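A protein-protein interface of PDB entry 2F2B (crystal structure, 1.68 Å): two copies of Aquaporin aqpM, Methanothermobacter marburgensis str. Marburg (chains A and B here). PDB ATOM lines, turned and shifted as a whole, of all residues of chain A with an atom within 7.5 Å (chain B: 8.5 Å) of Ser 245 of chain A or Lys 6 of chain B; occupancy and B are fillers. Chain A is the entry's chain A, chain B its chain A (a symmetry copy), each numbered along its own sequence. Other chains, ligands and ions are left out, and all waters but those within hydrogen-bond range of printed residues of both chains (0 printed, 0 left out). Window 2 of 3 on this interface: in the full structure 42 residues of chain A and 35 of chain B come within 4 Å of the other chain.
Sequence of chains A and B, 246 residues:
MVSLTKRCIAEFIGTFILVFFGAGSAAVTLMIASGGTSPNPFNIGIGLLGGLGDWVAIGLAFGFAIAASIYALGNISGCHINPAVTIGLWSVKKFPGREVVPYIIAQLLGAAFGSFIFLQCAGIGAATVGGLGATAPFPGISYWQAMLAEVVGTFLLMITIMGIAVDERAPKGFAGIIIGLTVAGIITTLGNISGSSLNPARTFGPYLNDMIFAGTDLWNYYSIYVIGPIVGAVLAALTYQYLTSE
The backbone carbonyl oxygen (O) of Tyr 242 of chain A lies within hydrogen-bond range of the side-chain amino group (NZ) of Lys 6 of chain B, 3.1 Å away.
The side-chain hydroxyl (OG) of Ser 245 of chain A lies within hydrogen-bond range of the side-chain amino group (NZ) of Lys 6 of chain B (2.8 Å).
OG1 of Thr 244 of chain A is in hydrogen-bond range of O of Tyr 240 of chain A (2.8 Å).
The backbone carbonyl oxygen of Tyr 242 of chain A lies within hydrogen-bond range of the side-chain hydroxyl of Ser 245 of chain A, 2.6 Å away.
O of Val 2 of chain B sits at hydrogen-bond distance from NE of Arg 7 of chain B, at 2.8 Å.
OG of Ser 3 of chain B lies within hydrogen-bond range of N of Lys 6 of chain B.
Thr 239 of chain A touches Ile 13 of chain B.
Ile 9 of chain B touches Tyr 242 of chain A (CD1 to OH, 3.8 Å).
O of Leu 243 of chain A touches CG1 of Val 2 of chain B, 3.8 Å away.
Lys 6 of chain B touches Leu 243 of chain A (O to CD2, 3.6 Å).
Leu 243 of chain A touches Ile 9 of chain B.
Ile 76 of chain B touches Leu 243 of chain A.
Thr 244 of chain A touches Ile 76 of chain B (CG2 to CD1, 3.9 Å).
Printed residues of chain B within 4 Å of Ser 245 of chain A: Lys 6 (2.8 Å).
Lys 6 of chain B touches just these residues of chain A: Tyr 242 (3.1 Å), Leu 243 (3.6 Å) and Ser 245 (2.8 Å).
Of the printed residues of chain A, Val 2 of chain B touches Leu 243.
Of the printed residues of chain A, Ile 9 of chain B touches Tyr 242 (3.8 Å) and Leu 243 (3.96 Å).
Of the printed residues of chain B, Thr 244 of chain A touches Ile 76.
Of the printed residues of chain B, Leu 243 of chain A touches Val 2, Lys 6, Ile 9 and Ile 76.
The nearest residue of chain A that does not touch Lys 6 of chain B is Thr 244 of chain A (5.3 Å).
The nearest printed residue of chain B that does not touch Thr 244 of chain A is Lys 6 of chain B (5.3 Å).
Printed residues of chain A that touch a printed residue of chain B: Thr 239, Tyr 242, Leu 243, Thr 244 and Ser 245.
Hydrophobic or aromatic side chains of chain A that line the printed part of chain B: Tyr 242 and Leu 243.
Printed residues of chain B that touch a printed residue of chain A: Val 2, Lys 6, Ile 9, Ile 13 and Ile 76.
Among the printed residues, 9 pairs touch across the chains.
No position is printed for both chains.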
ATOM      1  N   THR A 239     -23.168  -6.685 -35.247  1.00  0.00           N
ATOM      2  CA  THR A 239     -22.468  -5.931 -34.213  1.00  0.00           C
ATOM      3  C   THR A 239     -20.957  -6.063 -34.393  1.00  0.00           C
ATOM      4  O   THR A 239     -20.224  -5.079 -34.307  1.00  0.00           O
ATOM      5  CB  THR A 239     -22.848  -6.434 -32.801  1.00  0.00           C
ATOM      6  OG1 THR A 239     -24.242  -6.205 -32.573  1.00  0.00           O
ATOM      7  CG2 THR A 239     -22.039  -5.709 -31.735  1.00  0.00           C
ATOM      8  N   TYR A 240     -20.492  -7.282 -34.651  1.00  0.00           N
ATOM      9  CA  TYR A 240     -19.065  -7.502 -34.835  1.00  0.00           C
ATOM     10  C   TYR A 240     -18.568  -6.720 -36.048  1.00  0.00           C
ATOM     11  O   TYR A 240     -17.515  -6.084 -36.001  1.00  0.00           O
ATOM     12  CB  TYR A 240     -18.772  -8.991 -35.023  1.00  0.00           C
ATOM     13  CG  TYR A 240     -17.299  -9.313 -35.010  1.00  0.00           C
ATOM     14  CD1 TYR A 240     -16.553  -9.322 -36.191  1.00  0.00           C
ATOM     15  CD2 TYR A 240     -16.638  -9.570 -33.809  1.00  0.00           C
ATOM     16  CE1 TYR A 240     -15.183  -9.579 -36.173  1.00  0.00           C
ATOM     17  CE2 TYR A 240     -15.270  -9.826 -33.780  1.00  0.00           C
ATOM     18  CZ  TYR A 240     -14.551  -9.827 -34.962  1.00  0.00           C
ATOM     19  OH  TYR A 240     -13.198 -10.067 -34.933  1.00  0.00           O
ATOM     20  N   GLN A 241     -19.338  -6.776 -37.129  1.00  0.00           N
ATOM     21  CA  GLN A 241     -19.004  -6.076 -38.365  1.00  0.00           C
ATOM     22  C   GLN A 241     -18.867  -4.577 -38.102  1.00  0.00           C
ATOM     23  O   GLN A 241     -17.963  -3.923 -38.622  1.00  0.00           O
ATOM     24  CB  GLN A 241     -20.099  -6.333 -39.406  1.00  0.00           C
ATOM     25  CG  GLN A 241     -19.835  -5.750 -40.785  1.00  0.00           C
ATOM     26  CD  GLN A 241     -20.967  -6.042 -41.756  1.00  0.00           C
ATOM     27  OE1 GLN A 241     -22.099  -5.598 -41.561  1.00  0.00           O
ATOM     28  NE2 GLN A 241     -20.666  -6.799 -42.805  1.00  0.00           N
ATOM     29  N   TYR A 242     -19.771  -4.044 -37.287  1.00  0.00           N
ATOM     30  CA  TYR A 242     -19.763  -2.626 -36.944  1.00  0.00           C
ATOM     31  C   TYR A 242     -18.532  -2.240 -36.123  1.00  0.00           C
ATOM     32  O   TYR A 242     -17.838  -1.276 -36.447  1.00  0.00           O
ATOM     33  CB  TYR A 242     -21.034  -2.277 -36.162  1.00  0.00           C
ATOM     34  CG  TYR A 242     -20.976  -0.945 -35.447  1.00  0.00           C
ATOM     35  CD1 TYR A 242     -20.962   0.257 -36.157  1.00  0.00           C
ATOM     36  CD2 TYR A 242     -20.917  -0.890 -34.055  1.00  0.00           C
ATOM     37  CE1 TYR A 242     -20.891   1.484 -35.493  1.00  0.00           C
ATOM     38  CE2 TYR A 242     -20.844   0.327 -33.385  1.00  0.00           C
ATOM     39  CZ  TYR A 242     -20.833   1.508 -34.106  1.00  0.00           C
ATOM     40  OH  TYR A 242     -20.764   2.710 -33.435  1.00  0.00           O
ATOM     41  N   LEU A 243     -18.267  -2.996 -35.061  1.00  0.00           N
ATOM     42  CA  LEU A 243     -17.128  -2.725 -34.187  1.00  0.00           C
ATOM     43  C   LEU A 243     -15.772  -2.806 -34.883  1.00  0.00           C
ATOM     44  O   LEU A 243     -14.839  -2.087 -34.519  1.00  0.00           O
ATOM     45  CB  LEU A 243     -17.138  -3.688 -32.993  1.00  0.00           C
ATOM     46  CG  LEU A 243     -18.309  -3.559 -32.015  1.00  0.00           C
ATOM     47  CD1 LEU A 243     -18.200  -4.641 -30.941  1.00  0.00           C
ATOM     48  CD2 LEU A 243     -18.307  -2.168 -31.380  1.00  0.00           C
ATOM     49  N   THR A 244     -15.666  -3.675 -35.883  1.00  0.00           N
ATOM     50  CA  THR A 244     -14.412  -3.850 -36.605  1.00  0.00           C
ATOM     51  C   THR A 244     -14.385  -3.132 -37.950  1.00  0.00           C
ATOM     52  O   THR A 244     -13.428  -3.272 -38.708  1.00  0.00           O
ATOM     53  CB  THR A 244     -14.124  -5.342 -36.856  1.00  0.00           C
ATOM     54  OG1 THR A 244     -15.202  -5.914 -37.606  1.00  0.00           O
ATOM     55  CG2 THR A 244     -13.977  -6.090 -35.531  1.00  0.00           C
ATOM     56  N   SER A 245     -15.430  -2.366 -38.245  1.00  0.00           N
ATOM     57  CA  SER A 245     -15.503  -1.641 -39.511  1.00  0.00           C
ATOM     58  C   SER A 245     -14.538  -0.461 -39.519  1.00  0.00           C
ATOM     59  O   SER A 245     -14.206   0.089 -38.468  1.00  0.00           O
ATOM     60  CB  SER A 245     -16.930  -1.141 -39.758  1.00  0.00           C
ATOM     61  OG  SER A 245     -17.318  -0.187 -38.785  1.00  0.00           O
ATOM     62  N   MET B   1      -6.230   1.266 -32.811  1.00  0.00           N
ATOM     63  CA  MET B   1      -6.779   1.418 -34.188  1.00  0.00           C
ATOM     64  C   MET B   1      -8.285   1.657 -34.158  1.00  0.00           C
ATOM     65  O   MET B   1      -8.810   2.444 -34.942  1.00  0.00           O
ATOM     66  CB  MET B   1      -6.471   0.171 -35.020  1.00  0.00           C
ATOM     67  CG  MET B   1      -4.992  -0.030 -35.312  1.00  0.00           C
ATOM     68  SD  MET B   1      -4.323   1.215 -36.437  1.00  0.00           S
ATOM     69  CE  MET B   1      -4.186   0.268 -37.948  1.00  0.00           C
ATOM     70  N   VAL B   2      -8.977   0.972 -33.253  1.00  0.00           N
ATOM     71  CA  VAL B   2     -10.422   1.126 -33.125  1.00  0.00           C
ATOM     72  C   VAL B   2     -10.721   2.375 -32.298  1.00  0.00           C
ATOM     73  O   VAL B   2     -10.046   2.644 -31.304  1.00  0.00           O
ATOM     74  CB  VAL B   2     -11.056  -0.110 -32.441  1.00  0.00           C
ATOM     75  CG1 VAL B   2     -12.555   0.069 -32.313  1.00  0.00           C
ATOM     76  CG2 VAL B   2     -10.744  -1.362 -33.249  1.00  0.00           C
ATOM     77  N   SER B   3     -11.730   3.137 -32.713  1.00  0.00           N
ATOM     78  CA  SER B   3     -12.100   4.363 -32.007  1.00  0.00           C
ATOM     79  C   SER B   3     -12.485   4.085 -30.562  1.00  0.00           C
ATOM     80  O   SER B   3     -12.906   2.974 -30.223  1.00  0.00           O
ATOM     81  CB  SER B   3     -13.271   5.057 -32.705  1.00  0.00           C
ATOM     82  OG  SER B   3     -14.482   4.339 -32.520  1.00  0.00           O
ATOM     83  N   LEU B   4     -12.356   5.105 -29.718  1.00  0.00           N
ATOM     84  CA  LEU B   4     -12.699   4.979 -28.306  1.00  0.00           C
ATOM     85  C   LEU B   4     -14.187   4.687 -28.147  1.00  0.00           C
ATOM     86  O   LEU B   4     -14.591   3.964 -27.237  1.00  0.00           O
ATOM     87  CB  LEU B   4     -12.333   6.263 -27.554  1.00  0.00           C
ATOM     88  CG  LEU B   4     -12.576   6.298 -26.040  1.00  0.00           C
ATOM     89  CD1 LEU B   4     -11.838   5.149 -25.359  1.00  0.00           C
ATOM     90  CD2 LEU B   4     -12.097   7.637 -25.481  1.00  0.00           C
ATOM     91  N   THR B   5     -15.004   5.253 -29.030  1.00  0.00           N
ATOM     92  CA  THR B   5     -16.443   5.023 -28.973  1.00  0.00           C
ATOM     93  C   THR B   5     -16.746   3.535 -29.143  1.00  0.00           C
ATOM     94  O   THR B   5     -17.488   2.951 -28.355  1.00  0.00           O
ATOM     95  CB  THR B   5     -17.184   5.814 -30.075  1.00  0.00           C
ATOM     96  OG1 THR B   5     -17.088   7.216 -29.797  1.00  0.00           O
ATOM     97  CG2 THR B   5     -18.653   5.415 -30.127  1.00  0.00           C
ATOM     98  N   LYS B   6     -16.164   2.926 -30.168  1.00  0.00           N
ATOM     99  CA  LYS B   6     -16.383   1.506 -30.420  1.00  0.00           C
ATOM    100  C   LYS B   6     -15.745   0.638 -29.339  1.00  0.00           C
ATOM    101  O   LYS B   6     -16.278  -0.419 -28.987  1.00  0.00           O
ATOM    102  CB  LYS B   6     -15.841   1.131 -31.799  1.00  0.00           C
ATOM    103  CG  LYS B   6     -16.708   1.669 -32.932  1.00  0.00           C
ATOM    104  CD  LYS B   6     -16.123   1.353 -34.295  1.00  0.00           C
ATOM    105  CE  LYS B   6     -17.078   1.784 -35.401  1.00  0.00           C
ATOM    106  NZ  LYS B   6     -16.502   1.542 -36.751  1.00  0.00           N
ATOM    107  N   ARG B   7     -14.609   1.079 -28.810  1.00  0.00           N
ATOM    108  CA  ARG B   7     -13.938   0.323 -27.761  1.00  0.00           C
ATOM    109  C   ARG B   7     -14.751   0.355 -26.471  1.00  0.00           C
ATOM    110  O   ARG B   7     -14.787  -0.629 -25.732  1.00  0.00           O
ATOM    111  CB  ARG B   7     -12.520   0.858 -27.543  1.00  0.00           C
ATOM    112  CG  ARG B   7     -11.565   0.415 -28.647  1.00  0.00           C
ATOM    113  CD  ARG B   7     -10.122   0.758 -28.346  1.00  0.00           C
ATOM    114  NE  ARG B   7      -9.839   2.181 -28.511  1.00  0.00           N
ATOM    115  CZ  ARG B   7      -9.371   2.963 -27.547  1.00  0.00           C
ATOM    116  NH1 ARG B   7      -9.136   2.461 -26.341  1.00  0.00           N
ATOM    117  NH2 ARG B   7      -9.117   4.245 -27.791  1.00  0.00           N
ATOM    118  N   CYS B   8     -15.414   1.476 -26.201  1.00  0.00           N
ATOM    119  CA  CYS B   8     -16.246   1.577 -25.006  1.00  0.00           C
ATOM    120  C   CYS B   8     -17.490   0.709 -25.185  1.00  0.00           C
ATOM    121  O   CYS B   8     -17.974   0.101 -24.229  1.00  0.00           O
ATOM    122  CB  CYS B   8     -16.640   3.031 -24.738  1.00  0.00           C
ATOM    123  SG  CYS B   8     -15.323   4.001 -23.963  1.00  0.00           S
ATOM    124  N   ILE B   9     -18.012   0.651 -26.405  1.00  0.00           N
ATOM    125  CA  ILE B   9     -19.176  -0.188 -26.670  1.00  0.00           C
ATOM    126  C   ILE B   9     -18.761  -1.644 -26.425  1.00  0.00           C
ATOM    127  O   ILE B   9     -19.517  -2.427 -25.847  1.00  0.00           O
ATOM    128  CB  ILE B   9     -19.677  -0.025 -28.124  1.00  0.00           C
ATOM    129  CG1 ILE B   9     -20.270   1.373 -28.315  1.00  0.00           C
ATOM    130  CG2 ILE B   9     -20.726  -1.090 -28.441  1.00  0.00           C
ATOM    131  CD1 ILE B   9     -20.640   1.690 -29.760  1.00  0.00           C
ATOM    132  N   ALA B  10     -17.549  -1.992 -26.849  1.00  0.00           N
ATOM    133  CA  ALA B  10     -17.038  -3.347 -26.655  1.00  0.00           C
ATOM    134  C   ALA B  10     -16.896  -3.659 -25.163  1.00  0.00           C
ATOM    135  O   ALA B  10     -17.239  -4.752 -24.724  1.00  0.00           O
ATOM    136  CB  ALA B  10     -15.692  -3.510 -27.355  1.00  0.00           C
ATOM    137  N   GLU B  11     -16.386  -2.706 -24.387  1.00  0.00           N
ATOM    138  CA  GLU B  11     -16.233  -2.919 -22.946  1.00  0.00           C
ATOM    139  C   GLU B  11     -17.606  -3.099 -22.290  1.00  0.00           C
ATOM    140  O   GLU B  11     -17.758  -3.880 -21.351  1.00  0.00           O
ATOM    141  CB  GLU B  11     -15.487  -1.740 -22.305  1.00  0.00           C
ATOM    142  CG  GLU B  11     -13.994  -1.697 -22.625  1.00  0.00           C
ATOM    143  CD  GLU B  11     -13.231  -2.878 -22.039  1.00  0.00           C
ATOM    144  OE1 GLU B  11     -13.374  -3.134 -20.827  1.00  0.00           O
ATOM    145  OE2 GLU B  11     -12.482  -3.545 -22.786  1.00  0.00           O
ATOM    146  N   PHE B  12     -18.603  -2.373 -22.788  1.00  0.00           N
ATOM    147  CA  PHE B  12     -19.965  -2.470 -22.268  1.00  0.00           C
ATOM    148  C   PHE B  12     -20.496  -3.880 -22.534  1.00  0.00           C
ATOM    149  O   PHE B  12     -21.017  -4.542 -21.634  1.00  0.00           O
ATOM    150  CB  PHE B  12     -20.862  -1.427 -22.954  1.00  0.00           C
ATOM    151  CG  PHE B  12     -22.324  -1.532 -22.594  1.00  0.00           C
ATOM    152  CD1 PHE B  12     -23.150  -2.454 -23.232  1.00  0.00           C
ATOM    153  CD2 PHE B  12     -22.878  -0.691 -21.630  1.00  0.00           C
ATOM    154  CE1 PHE B  12     -24.512  -2.538 -22.916  1.00  0.00           C
ATOM    155  CE2 PHE B  12     -24.234  -0.764 -21.308  1.00  0.00           C
ATOM    156  CZ  PHE B  12     -25.052  -1.688 -21.952  1.00  0.00           C
ATOM    157  N   ILE B  13     -20.354  -4.333 -23.776  1.00  0.00           N
ATOM    158  CA  ILE B  13     -20.816  -5.663 -24.166  1.00  0.00           C
ATOM    159  C   ILE B  13     -20.097  -6.755 -23.375  1.00  0.00           C
ATOM    160  O   ILE B  13     -20.729  -7.689 -22.871  1.00  0.00           O
ATOM    161  CB  ILE B  13     -20.597  -5.899 -25.677  1.00  0.00           C
ATOM    162  CG1 ILE B  13     -21.524  -4.982 -26.479  1.00  0.00           C
ATOM    163  CG2 ILE B  13     -20.862  -7.365 -26.032  1.00  0.00           C
ATOM    164  CD1 ILE B  13     -21.235  -4.960 -27.969  1.00  0.00           C
ATOM    165  N   LEU B  73     -13.655  -9.747 -28.303  1.00  0.00           N
ATOM    166  CA  LEU B  73     -13.401  -8.316 -28.151  1.00  0.00           C
ATOM    167  C   LEU B  73     -11.978  -7.896 -27.821  1.00  0.00           C
ATOM    168  O   LEU B  73     -11.678  -6.697 -27.813  1.00  0.00           O
ATOM    169  CB  LEU B  73     -14.346  -7.767 -27.075  1.00  0.00           C
ATOM    170  CG  LEU B  73     -15.802  -8.210 -27.201  1.00  0.00           C
ATOM    171  CD1 LEU B  73     -16.552  -7.858 -25.927  1.00  0.00           C
ATOM    172  CD2 LEU B  73     -16.458  -7.559 -28.417  1.00  0.00           C
ATOM    173  N   ILE B  76     -10.347  -5.622 -30.138  1.00  0.00           N
ATOM    174  CA  ILE B  76     -11.084  -4.384 -30.320  1.00  0.00           C
ATOM    175  C   ILE B  76     -10.753  -3.383 -29.218  1.00  0.00           C
ATOM    176  O   ILE B  76     -10.167  -2.335 -29.487  1.00  0.00           O
ATOM    177  CB  ILE B  76     -12.609  -4.656 -30.358  1.00  0.00           C
ATOM    178  CG1 ILE B  76     -12.939  -5.539 -31.569  1.00  0.00           C
ATOM    179  CG2 ILE B  76     -13.382  -3.344 -30.441  1.00  0.00           C
ATOM    180  CD1 ILE B  76     -14.390  -5.976 -31.641  1.00  0.00           C
ATOM    181  N   SER B  77     -11.096  -3.717 -27.976  1.00  0.00           N
ATOM    182  CA  SER B  77     -10.851  -2.816 -26.853  1.00  0.00           C
ATOM    183  C   SER B  77      -9.773  -3.293 -25.892  1.00  0.00           C
ATOM    184  O   SER B  77      -9.316  -2.528 -25.040  1.00  0.00           O
ATOM    185  CB  SER B  77     -12.140  -2.621 -26.058  1.00  0.00           C
ATOM    186  OG  SER B  77     -12.504  -3.830 -25.400  1.00  0.00           O
ATOM    187  N   TYR B 103     -13.500   3.862 -19.945  1.00  0.00           N
ATOM    188  CA  TYR B 103     -13.623   2.405 -19.866  1.00  0.00           C
ATOM    189  C   TYR B 103     -14.406   1.966 -18.633  1.00  0.00           C
ATOM    190  O   TYR B 103     -15.286   1.110 -18.726  1.00  0.00           O
ATOM    191  CB  TYR B 103     -12.244   1.738 -19.838  1.00  0.00           C
ATOM    192  CG  TYR B 103     -11.736   1.278 -21.186  1.00  0.00           C
ATOM    193  CD1 TYR B 103     -11.018   0.088 -21.305  1.00  0.00           C
ATOM    194  CD2 TYR B 103     -11.946   2.039 -22.338  1.00  0.00           C
ATOM    195  CE1 TYR B 103     -10.518  -0.334 -22.532  1.00  0.00           C
ATOM    196  CE2 TYR B 103     -11.451   1.626 -23.572  1.00  0.00           C
ATOM    197  CZ  TYR B 103     -10.736   0.439 -23.662  1.00  0.00           C
ATOM    198  OH  TYR B 103     -10.228   0.030 -24.870  1.00  0.00           O
ATOM    199  N   ALA B 106     -18.131   2.555 -18.988  1.00  0.00           N
ATOM    200  CA  ALA B 106     -18.704   1.573 -19.903  1.00  0.00           C
ATOM    201  C   ALA B 106     -18.879   0.230 -19.200  1.00  0.00           C
ATOM    202  O   ALA B 106     -19.877  -0.459 -19.405  1.00  0.00           O
ATOM    203  CB  ALA B 106     -17.805   1.405 -21.131  1.00  0.00           C
